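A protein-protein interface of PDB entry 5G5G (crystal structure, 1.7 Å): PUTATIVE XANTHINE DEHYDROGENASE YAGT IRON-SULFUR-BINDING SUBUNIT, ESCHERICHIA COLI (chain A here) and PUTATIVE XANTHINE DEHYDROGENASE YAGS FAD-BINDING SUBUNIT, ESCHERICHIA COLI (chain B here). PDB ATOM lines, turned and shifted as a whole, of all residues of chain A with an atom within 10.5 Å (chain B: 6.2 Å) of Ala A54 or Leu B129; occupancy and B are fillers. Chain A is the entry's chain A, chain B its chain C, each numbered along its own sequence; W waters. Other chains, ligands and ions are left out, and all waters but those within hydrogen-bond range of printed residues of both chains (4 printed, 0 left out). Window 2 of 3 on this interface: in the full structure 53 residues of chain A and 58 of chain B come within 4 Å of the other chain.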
ATOM      1  N   PRO A  52      -9.418  -2.382 -30.575  1.00  0.00           N
ATOM      2  CA  PRO A  52      -9.377  -3.674 -29.864  1.00  0.00           C
ATOM      3  C   PRO A  52     -10.036  -3.602 -28.463  1.00  0.00           C
ATOM      4  O   PRO A  52     -11.011  -2.884 -28.304  1.00  0.00           O
ATOM      5  CB  PRO A  52      -7.865  -3.993 -29.807  1.00  0.00           C
ATOM      6  CG  PRO A  52      -7.289  -3.308 -31.009  1.00  0.00           C
ATOM      7  CD  PRO A  52      -8.161  -2.098 -31.300  1.00  0.00           C
ATOM      8  N   ALA A  53      -9.527  -4.345 -27.478  1.00  0.00           N
ATOM      9  CA  ALA A  53      -9.998  -4.273 -26.072  1.00  0.00           C
ATOM     10  C   ALA A  53      -9.195  -3.297 -25.160  1.00  0.00           C
ATOM     11  O   ALA A  53      -9.459  -3.217 -23.951  1.00  0.00           O
ATOM     12  CB  ALA A  53      -9.944  -5.671 -25.468  1.00  0.00           C
ATOM     13  N   ALA A  54      -8.191  -2.622 -25.723  1.00  0.00           N
ATOM     14  CA  ALA A  54      -7.293  -1.743 -24.966  1.00  0.00           C
ATOM     15  C   ALA A  54      -6.739  -0.652 -25.886  1.00  0.00           C
ATOM     16  O   ALA A  54      -6.796  -0.772 -27.120  1.00  0.00           O
ATOM     17  CB  ALA A  54      -6.159  -2.551 -24.314  1.00  0.00           C
ATOM     18  N   THR A  55      -6.300   0.452 -25.282  1.00  0.00           N
ATOM     19  CA  THR A  55      -5.578   1.510 -25.986  1.00  0.00           C
ATOM     20  C   THR A  55      -4.369   1.898 -25.100  1.00  0.00           C
ATOM     21  O   THR A  55      -4.483   1.859 -23.869  1.00  0.00           O
ATOM     22  CB  THR A  55      -6.514   2.718 -26.293  1.00  0.00           C
ATOM     23  OG1 THR A  55      -5.959   3.522 -27.326  1.00  0.00           O
ATOM     24  CG2 THR A  55      -6.863   3.547 -25.049  1.00  0.00           C
ATOM     25  N   PRO A  56      -3.202   2.198 -25.716  1.00  0.00           N
ATOM     26  CA  PRO A  56      -1.971   2.376 -24.899  1.00  0.00           C
ATOM     27  C   PRO A  56      -1.988   3.648 -24.036  1.00  0.00           C
ATOM     28  O   PRO A  56      -2.661   4.636 -24.377  1.00  0.00           O
ATOM     29  CB  PRO A  56      -0.854   2.485 -25.949  1.00  0.00           C
ATOM     30  CG  PRO A  56      -1.512   2.511 -27.300  1.00  0.00           C
ATOM     31  CD  PRO A  56      -2.933   2.094 -27.163  1.00  0.00           C
ATOM     32  N   ALA A  57      -1.251   3.600 -22.929  1.00  0.00           N
ATOM     33  CA  ALA A  57      -1.079   4.766 -22.066  1.00  0.00           C
ATOM     34  C   ALA A  57      -0.282   5.853 -22.760  1.00  0.00           C
ATOM     35  O   ALA A  57       0.578   5.540 -23.645  1.00  0.00           O
ATOM     36  CB  ALA A  57      -0.352   4.386 -20.791  1.00  0.00           C
ATOM     37  N   ARG A  79       0.937  12.747 -28.314  1.00  0.00           N
ATOM     38  CA  ARG A  79      -0.174  12.985 -29.225  1.00  0.00           C
ATOM     39  C   ARG A  79      -0.563  14.431 -29.256  1.00  0.00           C
ATOM     40  O   ARG A  79      -1.317  14.820 -30.173  1.00  0.00           O
ATOM     41  CB  ARG A  79      -1.412  12.202 -28.795  1.00  0.00           C
ATOM     42  CG  ARG A  79      -1.284  10.680 -28.903  1.00  0.00           C
ATOM     43  CD  ARG A  79      -2.480  10.003 -28.292  1.00  0.00           C
ATOM     44  NE  ARG A  79      -2.414   9.977 -26.834  1.00  0.00           N
ATOM     45  CZ  ARG A  79      -3.165   9.166 -26.061  1.00  0.00           C
ATOM     46  NH1 ARG A  79      -4.083   8.300 -26.603  1.00  0.00           N
ATOM     47  NH2 ARG A  79      -2.986   9.190 -24.727  1.00  0.00           N
ATOM     48  N   ASP B  67     -21.422  -1.401 -24.226  1.00  0.00           N
ATOM     49  CA  ASP B  67     -20.543  -1.926 -23.207  1.00  0.00           C
ATOM     50  C   ASP B  67     -19.400  -0.968 -23.011  1.00  0.00           C
ATOM     51  O   ASP B  67     -18.935  -0.334 -23.927  1.00  0.00           O
ATOM     52  CB  ASP B  67     -20.127  -3.310 -23.561  1.00  0.00           C
ATOM     53  CG  ASP B  67     -21.302  -4.240 -23.678  1.00  0.00           C
ATOM     54  OD1 ASP B  67     -22.072  -4.374 -22.657  1.00  0.00           O
ATOM     55  OD2 ASP B  67     -21.526  -4.780 -24.801  1.00  0.00           O
ATOM     56  N   THR B  68     -19.020  -0.781 -21.762  1.00  0.00           N
ATOM     57  CA  THR B  68     -18.116   0.310 -21.430  1.00  0.00           C
ATOM     58  C   THR B  68     -16.922  -0.150 -20.590  1.00  0.00           C
ATOM     59  O   THR B  68     -16.140   0.720 -20.188  1.00  0.00           O
ATOM     60  CB  THR B  68     -18.884   1.391 -20.633  1.00  0.00           C
ATOM     61  OG1 THR B  68     -19.376   0.774 -19.438  1.00  0.00           O
ATOM     62  CG2 THR B  68     -20.040   1.935 -21.451  1.00  0.00           C
ATOM     63  N   ALA B  70     -14.103  -1.797 -21.394  1.00  0.00           N
ATOM     64  CA  ALA B  70     -12.785  -1.486 -21.958  1.00  0.00           C
ATOM     65  C   ALA B  70     -12.446  -0.004 -21.852  1.00  0.00           C
ATOM     66  O   ALA B  70     -11.276   0.349 -21.586  1.00  0.00           O
ATOM     67  CB  ALA B  70     -12.677  -1.954 -23.402  1.00  0.00           C
ATOM     68  N   ALA B  71     -13.438   0.855 -22.109  1.00  0.00           N
ATOM     69  CA  ALA B  71     -13.274   2.280 -21.977  1.00  0.00           C
ATOM     70  C   ALA B  71     -12.987   2.679 -20.543  1.00  0.00           C
ATOM     71  O   ALA B  71     -12.115   3.475 -20.289  1.00  0.00           O
ATOM     72  CB  ALA B  71     -14.478   3.001 -22.496  1.00  0.00           C
ATOM     73  N   ALA B  74      -9.427   2.186 -19.649  1.00  0.00           N
ATOM     74  CA  ALA B  74      -8.439   2.892 -20.469  1.00  0.00           C
ATOM     75  C   ALA B  74      -7.723   3.969 -19.626  1.00  0.00           C
ATOM     76  O   ALA B  74      -8.235   4.419 -18.586  1.00  0.00           O
ATOM     77  CB  ALA B  74      -9.064   3.455 -21.709  1.00  0.00           C
ATOM     78  N   PRO B  75      -6.494   4.342 -20.039  1.00  0.00           N
ATOM     79  CA  PRO B  75      -5.662   5.287 -19.315  1.00  0.00           C
ATOM     80  C   PRO B  75      -6.371   6.592 -19.058  1.00  0.00           C
ATOM     81  O   PRO B  75      -6.968   7.190 -19.983  1.00  0.00           O
ATOM     82  CB  PRO B  75      -4.470   5.467 -20.268  1.00  0.00           C
ATOM     83  CG  PRO B  75      -4.371   4.113 -20.893  1.00  0.00           C
ATOM     84  CD  PRO B  75      -5.767   3.776 -21.189  1.00  0.00           C
ATOM     85  N   ARG B 124     -10.489  10.933 -25.886  1.00  0.00           N
ATOM     86  CA  ARG B 124     -10.677  10.564 -27.276  1.00  0.00           C
ATOM     87  C   ARG B 124     -10.326   9.090 -27.540  1.00  0.00           C
ATOM     88  O   ARG B 124     -11.125   8.354 -28.166  1.00  0.00           O
ATOM     89  CB  ARG B 124      -9.876  11.492 -28.203  1.00  0.00           C
ATOM     90  CG  ARG B 124     -10.074  11.127 -29.670  1.00  0.00           C
ATOM     91  CD  ARG B 124      -9.381  12.139 -30.565  1.00  0.00           C
ATOM     92  NE  ARG B 124      -7.988  12.252 -30.205  1.00  0.00           N
ATOM     93  CZ  ARG B 124      -7.157  13.227 -30.568  1.00  0.00           C
ATOM     94  NH1 ARG B 124      -7.579  14.225 -31.328  1.00  0.00           N
ATOM     95  NH2 ARG B 124      -5.904  13.192 -30.156  1.00  0.00           N
ATOM     96  N   ALA B 125      -9.138   8.681 -27.079  1.00  0.00           N
ATOM     97  CA  ALA B 125      -8.664   7.322 -27.256  1.00  0.00           C
ATOM     98  C   ALA B 125      -9.591   6.320 -26.591  1.00  0.00           C
ATOM     99  O   ALA B 125      -9.855   5.241 -27.204  1.00  0.00           O
ATOM    100  CB  ALA B 125      -7.248   7.170 -26.759  1.00  0.00           C
ATOM    101  N   ALA B 126     -10.065   6.631 -25.379  1.00  0.00           N
ATOM    102  CA  ALA B 126     -10.970   5.727 -24.669  1.00  0.00           C
ATOM    103  C   ALA B 126     -12.342   5.602 -25.346  1.00  0.00           C
ATOM    104  O   ALA B 126     -12.939   4.534 -25.333  1.00  0.00           O
ATOM    105  CB  ALA B 126     -11.126   6.117 -23.194  1.00  0.00           C
ATOM    106  N   ALA B 127     -12.799   6.676 -25.951  1.00  0.00           N
ATOM    107  CA  ALA B 127     -14.091   6.682 -26.648  1.00  0.00           C
ATOM    108  C   ALA B 127     -14.122   5.654 -27.782  1.00  0.00           C
ATOM    109  O   ALA B 127     -15.174   5.053 -27.994  1.00  0.00           O
ATOM    110  CB  ALA B 127     -14.419   8.075 -27.146  1.00  0.00           C
ATOM    111  N   SER B 128     -12.996   5.405 -28.476  1.00  0.00           N
ATOM    112  CA  SER B 128     -12.927   4.366 -29.508  1.00  0.00           C
ATOM    113  C   SER B 128     -13.186   2.992 -28.986  1.00  0.00           C
ATOM    114  O   SER B 128     -13.427   2.108 -29.754  1.00  0.00           O
ATOM    115  CB  SER B 128     -11.511   4.260 -30.145  1.00  0.00           C
ATOM    116  OG  SER B 128     -11.128   5.543 -30.464  1.00  0.00           O
ATOM    117  N   LEU B 129     -12.987   2.796 -27.688  1.00  0.00           N
ATOM    118  CA  LEU B 129     -13.193   1.490 -27.076  1.00  0.00           C
ATOM    119  C   LEU B 129     -14.640   1.183 -26.625  1.00  0.00           C
ATOM    120  O   LEU B 129     -14.908   0.045 -26.257  1.00  0.00           O
ATOM    121  CB  LEU B 129     -12.267   1.318 -25.872  1.00  0.00           C
ATOM    122  CG  LEU B 129     -10.789   1.564 -26.149  1.00  0.00           C
ATOM    123  CD1 LEU B 129      -9.944   1.319 -24.899  1.00  0.00           C
ATOM    124  CD2 LEU B 129     -10.349   0.664 -27.271  1.00  0.00           C
ATOM    125  N   VAL B 130     -15.528   2.167 -26.637  1.00  0.00           N
ATOM    126  CA  VAL B 130     -16.898   1.940 -26.226  1.00  0.00           C
ATOM    127  C   VAL B 130     -17.514   0.974 -27.263  1.00  0.00           C
ATOM    128  O   VAL B 130     -17.451   1.268 -28.437  1.00  0.00           O
ATOM    129  CB  VAL B 130     -17.660   3.264 -26.131  1.00  0.00           C
ATOM    130  CG1 VAL B 130     -19.156   3.050 -25.923  1.00  0.00           C
ATOM    131  CG2 VAL B 130     -17.090   4.078 -24.973  1.00  0.00           C
ATOM    132  N   GLN B 131     -18.125  -0.109 -26.814  1.00  0.00           N
ATOM    133  CA  GLN B 131     -18.575  -1.192 -27.706  1.00  0.00           C
ATOM    134  C   GLN B 131     -20.090  -1.036 -27.854  1.00  0.00           C
ATOM    135  O   GLN B 131     -20.848  -1.417 -26.982  1.00  0.00           O
ATOM    136  CB  GLN B 131     -18.155  -2.530 -27.090  1.00  0.00           C
ATOM    137  CG  GLN B 131     -18.634  -3.781 -27.804  1.00  0.00           C
ATOM    138  CD  GLN B 131     -18.207  -5.084 -27.102  1.00  0.00           C
ATOM    139  OE1 GLN B 131     -17.003  -5.366 -26.995  1.00  0.00           O
ATOM    140  NE2 GLN B 131     -19.182  -5.882 -26.601  1.00  0.00           N
HETATM  141  O   HOH W   1     -13.606  -2.052 -27.390  1.00  0.00           O
HETATM  142  O   HOH W   2      -8.052   4.177 -28.968  1.00  0.00           O
HETATM  143  O   HOH W   3      -9.129  -1.175 -21.832  1.00  0.00           O
HETATM  144  O   HOH W   4      -3.975  15.121 -30.593  1.00  0.00           O
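Among the printed residues, pairs that only touch across the chains: Pro A52 with Leu B129, Ala A53 with Ala B70, Ala A54 with Leu B129, Thr A55 with Pro B75, Thr A55 with Ala B125, Thr A55 with Leu B129, Pro A56 with Pro B75, Ala A57 with Pro B75 and Arg A79 with Ala B125.
Of the printed residues of chain B, Ala A53 touches Ala B70 (3.5 Å).
Of the printed residues of chain B, Ala A54 touches Leu B129.
Of chain A, only Ala A53 (3.5 Å) comes within 4 Å of Ala B70.
Ala B74 touches none of the printed residues of chain A.
Printed residues of chain A within 4 Å of Pro B75: Thr A55, Pro A56 and Ala A57.
No residue of chain A comes within 4 Å of Ala B126.
No residue of chain A comes within 4 Å of Ala B127.
Ser B128 touches none of the printed residues of chain A.
Of chain A, only Pro A52 (3.8 Å), Ala A54 (3.8 Å) and Thr A55 (3.8 Å) come within 4 Å of Leu B129.
No residue of chain A comes within 4 Å of Val B130.
The nearest residue of chain A that does not touch Leu B129 is Ala A53 (4.6 Å).
The nearest printed residue of chain B that does not touch Pro A56 is Ala B125 (5.8 Å).
Of the 14 printed residues of chain B, 4 touch a printed residue of chain A.
Hydrophobic or aromatic side chains of chain B within 4 Å of the printed part of chain A: Ala B70, Pro B75, Ala B125 and Leu B129.
Of the 7 printed residues of chain A, 7 touch a printed residue of chain B.
Among the printed residues, no Asp or Glu carboxylate lies within 4 Å of a Lys or Arg side-chain nitrogen of the other chain.
Water W3 bridges O of Ala B70 and O of Ala A53.
Water W4 lies within hydrogen-bond range of O of Arg A79 (2.7 Å) and NH2 of Arg B124 (2.8 Å).
Water W1 bridges O of Leu B129 and O of Pro A52.
Water W2 lies within hydrogen-bond range of the backbone carbonyl oxygen (O) of Ala B125 and the side-chain hydroxyl (OG1) of Thr A55.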
